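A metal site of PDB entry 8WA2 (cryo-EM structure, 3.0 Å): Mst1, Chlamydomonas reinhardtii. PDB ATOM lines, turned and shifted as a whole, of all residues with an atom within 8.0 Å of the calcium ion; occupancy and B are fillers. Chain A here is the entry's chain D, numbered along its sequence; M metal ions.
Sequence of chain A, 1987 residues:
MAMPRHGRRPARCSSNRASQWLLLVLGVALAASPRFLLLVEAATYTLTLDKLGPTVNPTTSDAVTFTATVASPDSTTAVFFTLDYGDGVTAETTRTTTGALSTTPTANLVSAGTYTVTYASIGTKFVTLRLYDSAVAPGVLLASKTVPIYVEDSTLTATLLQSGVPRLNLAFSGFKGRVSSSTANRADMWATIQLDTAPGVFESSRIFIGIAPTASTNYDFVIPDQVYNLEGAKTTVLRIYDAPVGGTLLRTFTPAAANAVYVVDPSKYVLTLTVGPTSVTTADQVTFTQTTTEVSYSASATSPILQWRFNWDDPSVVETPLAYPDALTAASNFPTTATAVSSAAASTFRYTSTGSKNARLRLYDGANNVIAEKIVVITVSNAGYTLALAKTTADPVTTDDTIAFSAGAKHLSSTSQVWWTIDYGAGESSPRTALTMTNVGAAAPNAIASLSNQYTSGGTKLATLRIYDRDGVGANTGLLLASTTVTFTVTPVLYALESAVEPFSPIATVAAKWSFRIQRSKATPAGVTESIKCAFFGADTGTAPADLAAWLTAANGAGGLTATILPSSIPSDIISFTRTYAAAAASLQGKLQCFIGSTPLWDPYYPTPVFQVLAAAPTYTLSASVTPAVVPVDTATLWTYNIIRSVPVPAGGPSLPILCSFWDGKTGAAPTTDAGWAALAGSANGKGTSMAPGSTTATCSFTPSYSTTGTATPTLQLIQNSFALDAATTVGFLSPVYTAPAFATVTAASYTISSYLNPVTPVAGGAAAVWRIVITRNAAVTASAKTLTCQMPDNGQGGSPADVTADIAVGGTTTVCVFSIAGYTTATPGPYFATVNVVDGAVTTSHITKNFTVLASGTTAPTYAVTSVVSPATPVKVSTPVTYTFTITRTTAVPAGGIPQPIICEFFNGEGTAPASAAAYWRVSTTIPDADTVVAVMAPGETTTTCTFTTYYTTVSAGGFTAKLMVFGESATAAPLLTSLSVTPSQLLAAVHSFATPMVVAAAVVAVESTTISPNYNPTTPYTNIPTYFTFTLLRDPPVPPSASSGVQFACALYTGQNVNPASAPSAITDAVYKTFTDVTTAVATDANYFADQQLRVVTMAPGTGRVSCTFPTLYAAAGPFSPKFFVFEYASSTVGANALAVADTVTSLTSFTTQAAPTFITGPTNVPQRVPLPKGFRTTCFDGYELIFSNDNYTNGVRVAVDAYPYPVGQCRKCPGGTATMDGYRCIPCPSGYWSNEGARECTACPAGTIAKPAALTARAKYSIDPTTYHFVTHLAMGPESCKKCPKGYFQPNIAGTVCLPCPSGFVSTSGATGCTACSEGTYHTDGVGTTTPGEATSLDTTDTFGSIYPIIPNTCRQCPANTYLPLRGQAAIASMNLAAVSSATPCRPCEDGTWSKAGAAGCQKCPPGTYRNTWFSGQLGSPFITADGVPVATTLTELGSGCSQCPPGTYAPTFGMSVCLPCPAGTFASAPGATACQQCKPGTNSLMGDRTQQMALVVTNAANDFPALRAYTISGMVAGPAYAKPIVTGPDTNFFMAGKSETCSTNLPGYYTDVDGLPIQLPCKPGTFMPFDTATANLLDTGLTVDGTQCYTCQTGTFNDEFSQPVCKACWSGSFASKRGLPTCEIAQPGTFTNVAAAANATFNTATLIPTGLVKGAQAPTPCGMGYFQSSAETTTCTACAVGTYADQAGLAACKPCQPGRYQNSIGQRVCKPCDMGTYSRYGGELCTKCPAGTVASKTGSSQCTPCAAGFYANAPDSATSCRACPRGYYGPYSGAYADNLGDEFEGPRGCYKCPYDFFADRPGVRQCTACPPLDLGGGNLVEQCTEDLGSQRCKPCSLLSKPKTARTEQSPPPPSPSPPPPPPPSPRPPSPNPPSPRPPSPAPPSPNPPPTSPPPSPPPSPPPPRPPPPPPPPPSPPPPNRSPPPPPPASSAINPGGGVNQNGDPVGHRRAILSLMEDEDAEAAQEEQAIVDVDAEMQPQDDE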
ATOM      1  N   ILE A 904      24.513 -20.681  19.692  1.00  0.00           N
ATOM      2  CA  ILE A 904      23.416 -20.089  18.939  1.00  0.00           C
ATOM      3  C   ILE A 904      23.620 -18.582  18.925  1.00  0.00           C
ATOM      4  O   ILE A 904      23.737 -17.957  19.997  1.00  0.00           O
ATOM      5  CB  ILE A 904      22.057 -20.458  19.539  1.00  0.00           C
ATOM      6  CG1 ILE A 904      21.722 -21.918  19.243  1.00  0.00           C
ATOM      7  CG2 ILE A 904      20.975 -19.535  19.011  1.00  0.00           C
ATOM      8  CD1 ILE A 904      20.583 -22.461  20.071  1.00  0.00           C
ATOM      9  N   CYS A 905      23.655 -17.995  17.735  1.00  0.00           N
ATOM     10  CA  CYS A 905      23.722 -16.545  17.573  1.00  0.00           C
ATOM     11  C   CYS A 905      22.319 -16.035  17.245  1.00  0.00           C
ATOM     12  O   CYS A 905      21.677 -16.535  16.316  1.00  0.00           O
ATOM     13  CB  CYS A 905      24.712 -16.167  16.473  1.00  0.00           C
ATOM     14  SG  CYS A 905      26.440 -16.618  16.774  1.00  0.00           S
ATOM     15  N   GLU A 906      21.850 -15.058  18.007  1.00  0.00           N
ATOM     16  CA  GLU A 906      20.561 -14.425  17.792  1.00  0.00           C
ATOM     17  C   GLU A 906      20.775 -12.938  17.558  1.00  0.00           C
ATOM     18  O   GLU A 906      21.453 -12.267  18.347  1.00  0.00           O
ATOM     19  CB  GLU A 906      19.626 -14.665  18.992  1.00  0.00           C
ATOM     20  CG  GLU A 906      19.342 -16.136  19.253  1.00  0.00           C
ATOM     21  CD  GLU A 906      18.350 -16.349  20.380  1.00  0.00           C
ATOM     22  OE1 GLU A 906      18.481 -15.684  21.425  1.00  0.00           O
ATOM     23  OE2 GLU A 906      17.435 -17.187  20.217  1.00  0.00           O
ATOM     24  N   PHE A 907      20.185 -12.414  16.488  1.00  0.00           N
ATOM     25  CA  PHE A 907      20.520 -11.096  15.970  1.00  0.00           C
ATOM     26  C   PHE A 907      19.298 -10.189  15.993  1.00  0.00           C
ATOM     27  O   PHE A 907      18.166 -10.630  15.762  1.00  0.00           O
ATOM     28  CB  PHE A 907      21.058 -11.210  14.536  1.00  0.00           C
ATOM     29  CG  PHE A 907      21.191  -9.900  13.829  1.00  0.00           C
ATOM     30  CD1 PHE A 907      22.265  -9.073  14.085  1.00  0.00           C
ATOM     31  CD2 PHE A 907      20.251  -9.508  12.895  1.00  0.00           C
ATOM     32  CE1 PHE A 907      22.400  -7.862  13.429  1.00  0.00           C
ATOM     33  CE2 PHE A 907      20.378  -8.296  12.237  1.00  0.00           C
ATOM     34  CZ  PHE A 907      21.457  -7.477  12.502  1.00  0.00           C
ATOM     35  N   TYR A 921      16.656 -12.609  25.272  1.00  0.00           N
ATOM     36  CA  TYR A 921      16.786 -12.630  23.814  1.00  0.00           C
ATOM     37  C   TYR A 921      16.239 -13.899  23.181  1.00  0.00           C
ATOM     38  O   TYR A 921      16.246 -14.015  21.956  1.00  0.00           O
ATOM     39  CB  TYR A 921      18.248 -12.441  23.410  1.00  0.00           C
ATOM     40  CG  TYR A 921      18.574 -11.081  22.840  1.00  0.00           C
ATOM     41  CD1 TYR A 921      17.928 -10.622  21.695  1.00  0.00           C
ATOM     42  CD2 TYR A 921      19.536 -10.270  23.410  1.00  0.00           C
ATOM     43  CE1 TYR A 921      18.239  -9.388  21.158  1.00  0.00           C
ATOM     44  CE2 TYR A 921      19.842  -9.035  22.886  1.00  0.00           C
ATOM     45  CZ  TYR A 921      19.187  -8.596  21.762  1.00  0.00           C
ATOM     46  OH  TYR A 921      19.493  -7.361  21.238  1.00  0.00           O
ATOM     47  N   TRP A 922      15.771 -14.853  23.991  1.00  0.00           N
ATOM     48  CA  TRP A 922      15.213 -16.104  23.488  1.00  0.00           C
ATOM     49  C   TRP A 922      13.824 -15.835  22.917  1.00  0.00           C
ATOM     50  O   TRP A 922      12.797 -16.089  23.548  1.00  0.00           O
ATOM     51  CB  TRP A 922      15.179 -17.156  24.580  1.00  0.00           C
ATOM     52  CG  TRP A 922      16.080 -18.320  24.320  1.00  0.00           C
ATOM     53  CD1 TRP A 922      17.205 -18.654  25.015  1.00  0.00           C
ATOM     54  CD2 TRP A 922      15.937 -19.312  23.291  1.00  0.00           C
ATOM     55  NE1 TRP A 922      17.778 -19.789  24.485  1.00  0.00           N
ATOM     56  CE2 TRP A 922      17.019 -20.213  23.429  1.00  0.00           C
ATOM     57  CE3 TRP A 922      15.004 -19.528  22.284  1.00  0.00           C
ATOM     58  CZ2 TRP A 922      17.182 -21.310  22.586  1.00  0.00           C
ATOM     59  CZ3 TRP A 922      15.170 -20.611  21.440  1.00  0.00           C
ATOM     60  CH2 TRP A 922      16.257 -21.491  21.601  1.00  0.00           C
ATOM     61  N   ARG A 923      13.795 -15.298  21.708  1.00  0.00           N
ATOM     62  CA  ARG A 923      12.538 -15.055  21.026  1.00  0.00           C
ATOM     63  C   ARG A 923      11.926 -16.356  20.538  1.00  0.00           C
ATOM     64  O   ARG A 923      12.576 -17.413  20.516  1.00  0.00           O
ATOM     65  CB  ARG A 923      12.740 -14.096  19.848  1.00  0.00           C
ATOM     66  CG  ARG A 923      12.581 -12.624  20.192  1.00  0.00           C
ATOM     67  CD  ARG A 923      13.871 -12.040  20.722  1.00  0.00           C
ATOM     68  NE  ARG A 923      15.019 -12.446  19.918  1.00  0.00           N
ATOM     69  CZ  ARG A 923      15.599 -11.672  18.999  1.00  0.00           C
ATOM     70  NH1 ARG A 923      15.164 -10.454  18.733  1.00  0.00           N
ATOM     71  NH2 ARG A 923      16.645 -12.156  18.336  1.00  0.00           N
ATOM     72  N   VAL A 924      10.652 -16.283  20.152  1.00  0.00           N
ATOM     73  CA  VAL A 924       9.989 -17.452  19.579  1.00  0.00           C
ATOM     74  C   VAL A 924      10.566 -17.733  18.191  1.00  0.00           C
ATOM     75  O   VAL A 924      11.034 -16.821  17.487  1.00  0.00           O
ATOM     76  CB  VAL A 924       8.472 -17.236  19.513  1.00  0.00           C
ATOM     77  CG1 VAL A 924       7.915 -16.964  20.901  1.00  0.00           C
ATOM     78  CG2 VAL A 924       8.124 -16.091  18.571  1.00  0.00           C
ATOM     79  N   SER A 925      10.552 -19.007  17.799  1.00  0.00           N
ATOM     80  CA  SER A 925      11.062 -19.407  16.500  1.00  0.00           C
ATOM     81  C   SER A 925      10.530 -20.780  16.155  1.00  0.00           C
ATOM     82  O   SER A 925      10.704 -21.728  16.929  1.00  0.00           O
ATOM     83  CB  SER A 925      12.600 -19.413  16.485  1.00  0.00           C
ATOM     84  OG  SER A 925      13.117 -18.101  16.544  1.00  0.00           O
ATOM     85  N   THR A 926       9.863 -20.897  15.000  1.00  0.00           N
ATOM     86  CA  THR A 926       9.389 -22.200  14.543  1.00  0.00           C
ATOM     87  C   THR A 926      10.526 -23.035  13.963  1.00  0.00           C
ATOM     88  O   THR A 926      10.538 -24.267  14.123  1.00  0.00           O
ATOM     89  CB  THR A 926       8.294 -22.019  13.494  1.00  0.00           C
ATOM     90  OG1 THR A 926       8.757 -21.169  12.449  1.00  0.00           O
ATOM     91  CG2 THR A 926       7.049 -21.412  14.127  1.00  0.00           C
ATOM     92  N   THR A 927      11.489 -22.404  13.302  1.00  0.00           N
ATOM     93  CA  THR A 927      12.644 -23.078  12.725  1.00  0.00           C
ATOM     94  C   THR A 927      13.907 -22.405  13.242  1.00  0.00           C
ATOM     95  O   THR A 927      14.002 -21.177  13.230  1.00  0.00           O
ATOM     96  CB  THR A 927      12.610 -23.058  11.202  1.00  0.00           C
ATOM     97  OG1 THR A 927      12.129 -21.781  10.752  1.00  0.00           O
ATOM     98  CG2 THR A 927      11.685 -24.143  10.676  1.00  0.00           C
ATOM     99  N   ILE A 928      14.864 -23.215  13.676  1.00  0.00           N
ATOM    100  CA  ILE A 928      16.075 -22.662  14.301  1.00  0.00           C
ATOM    101  C   ILE A 928      16.904 -21.835  13.329  1.00  0.00           C
ATOM    102  O   ILE A 928      17.295 -20.715  13.686  1.00  0.00           O
ATOM    103  CB  ILE A 928      16.883 -23.798  14.966  1.00  0.00           C
ATOM    104  CG1 ILE A 928      15.964 -24.710  15.770  1.00  0.00           C
ATOM    105  CG2 ILE A 928      17.961 -23.202  15.865  1.00  0.00           C
ATOM    106  CD1 ILE A 928      15.213 -24.012  16.880  1.00  0.00           C
ATOM    107  N   PRO A 929      17.221 -22.309  12.103  1.00  0.00           N
ATOM    108  CA  PRO A 929      18.025 -21.470  11.205  1.00  0.00           C
ATOM    109  C   PRO A 929      17.181 -20.475  10.416  1.00  0.00           C
ATOM    110  O   PRO A 929      17.164 -20.474   9.176  1.00  0.00           O
ATOM    111  CB  PRO A 929      18.706 -22.511  10.302  1.00  0.00           C
ATOM    112  CG  PRO A 929      18.252 -23.872  10.783  1.00  0.00           C
ATOM    113  CD  PRO A 929      16.987 -23.637  11.528  1.00  0.00           C
ATOM    114  N   ASP A 930      16.469 -19.611  11.132  1.00  0.00           N
ATOM    115  CA  ASP A 930      15.669 -18.575  10.506  1.00  0.00           C
ATOM    116  C   ASP A 930      16.514 -17.323  10.306  1.00  0.00           C
ATOM    117  O   ASP A 930      17.743 -17.344  10.441  1.00  0.00           O
ATOM    118  CB  ASP A 930      14.401 -18.318  11.331  1.00  0.00           C
ATOM    119  CG  ASP A 930      14.694 -17.979  12.779  1.00  0.00           C
ATOM    120  OD1 ASP A 930      15.829 -17.565  13.088  1.00  0.00           O
ATOM    121  OD2 ASP A 930      13.777 -18.128  13.621  1.00  0.00           O
ATOM    122  N   ALA A 931      15.864 -16.200   9.981  1.00  0.00           N
ATOM    123  CA  ALA A 931      16.600 -14.979   9.656  1.00  0.00           C
ATOM    124  C   ALA A 931      17.317 -14.384  10.859  1.00  0.00           C
ATOM    125  O   ALA A 931      18.335 -13.715  10.671  1.00  0.00           O
ATOM    126  CB  ALA A 931      15.640 -13.945   9.058  1.00  0.00           C
ATOM    127  N   ASP A 932      16.816 -14.599  12.078  1.00  0.00           N
ATOM    128  CA  ASP A 932      17.384 -13.964  13.265  1.00  0.00           C
ATOM    129  C   ASP A 932      17.994 -14.984  14.230  1.00  0.00           C
ATOM    130  O   ASP A 932      18.187 -14.666  15.406  1.00  0.00           O
ATOM    131  CB  ASP A 932      16.327 -13.128  13.985  1.00  0.00           C
ATOM    132  CG  ASP A 932      15.173 -13.959  14.511  1.00  0.00           C
ATOM    133  OD1 ASP A 932      14.862 -14.994  13.891  1.00  0.00           O
ATOM    134  OD2 ASP A 932      14.591 -13.584  15.547  1.00  0.00           O
ATOM    135  N   THR A 933      18.294 -16.191  13.754  1.00  0.00           N
ATOM    136  CA  THR A 933      18.928 -17.202  14.591  1.00  0.00           C
ATOM    137  C   THR A 933      19.748 -18.139  13.722  1.00  0.00           C
ATOM    138  O   THR A 933      19.240 -18.671  12.736  1.00  0.00           O
ATOM    139  CB  THR A 933      17.896 -18.008  15.388  1.00  0.00           C
ATOM    140  OG1 THR A 933      16.794 -17.174  15.749  1.00  0.00           O
ATOM    141  CG2 THR A 933      18.512 -18.582  16.642  1.00  0.00           C
ATOM    142  N   VAL A 934      21.013 -18.325  14.096  1.00  0.00           N
ATOM    143  CA  VAL A 934      21.889 -19.279  13.426  1.00  0.00           C
ATOM    144  C   VAL A 934      22.577 -20.137  14.467  1.00  0.00           C
ATOM    145  O   VAL A 934      22.706 -19.747  15.640  1.00  0.00           O
ATOM    146  CB  VAL A 934      22.922 -18.576  12.501  1.00  0.00           C
ATOM    147  CG1 VAL A 934      24.218 -18.324  13.240  1.00  0.00           C
ATOM    148  CG2 VAL A 934      23.163 -19.405  11.249  1.00  0.00           C
ATOM    149  N   PHE A 949      24.833 -13.599   9.201  1.00  0.00           N
ATOM    150  CA  PHE A 949      23.427 -13.234   9.112  1.00  0.00           C
ATOM    151  C   PHE A 949      23.193 -12.307   7.922  1.00  0.00           C
ATOM    152  O   PHE A 949      24.092 -11.563   7.517  1.00  0.00           O
ATOM    153  CB  PHE A 949      22.933 -12.550  10.399  1.00  0.00           C
ATOM    154  CG  PHE A 949      22.824 -13.478  11.563  1.00  0.00           C
ATOM    155  CD1 PHE A 949      21.656 -14.184  11.806  1.00  0.00           C
ATOM    156  CD2 PHE A 949      23.897 -13.652  12.432  1.00  0.00           C
ATOM    157  CE1 PHE A 949      21.554 -15.036  12.885  1.00  0.00           C
ATOM    158  CE2 PHE A 949      23.805 -14.505  13.514  1.00  0.00           C
ATOM    159  CZ  PHE A 949      22.633 -15.197  13.740  1.00  0.00           C
HETATM  160 CA    CA M   1      14.586 -16.815  15.358  1.00  0.00          CA
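Within 4 Å of the calcium ion: Ser 925, Asp 930, Asp 932 and Thr 933.
Along chain A the residues within 4 Å of the calcium ion span positions 925 to 933.
The nearest printed residue that does not touch the calcium ion is Val 924 (4.1 Å).
NH2 of Arg 923 is in salt-bridge range of OD2 of Asp 932, 3.7 Å away.
The backbone carbonyl oxygen of Asp 932 is in hydrogen-bond range of the backbone NH of Phe 907, at 3.2 Å.
The side-chain hydroxyl (OG1) of Thr 933 binds the calcium ion.
OG of Ser 925 binds the calcium ion, at 2.3 Å.
The side-chain carboxylate (OD2) of Asp 930 is bound to the calcium ion.
The calcium ion is bound by OD1 of Asp 932, 2.4 Å away.
The side-chain carboxylate (OD1) of Asp 930 binds the calcium ion (2.7 Å).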
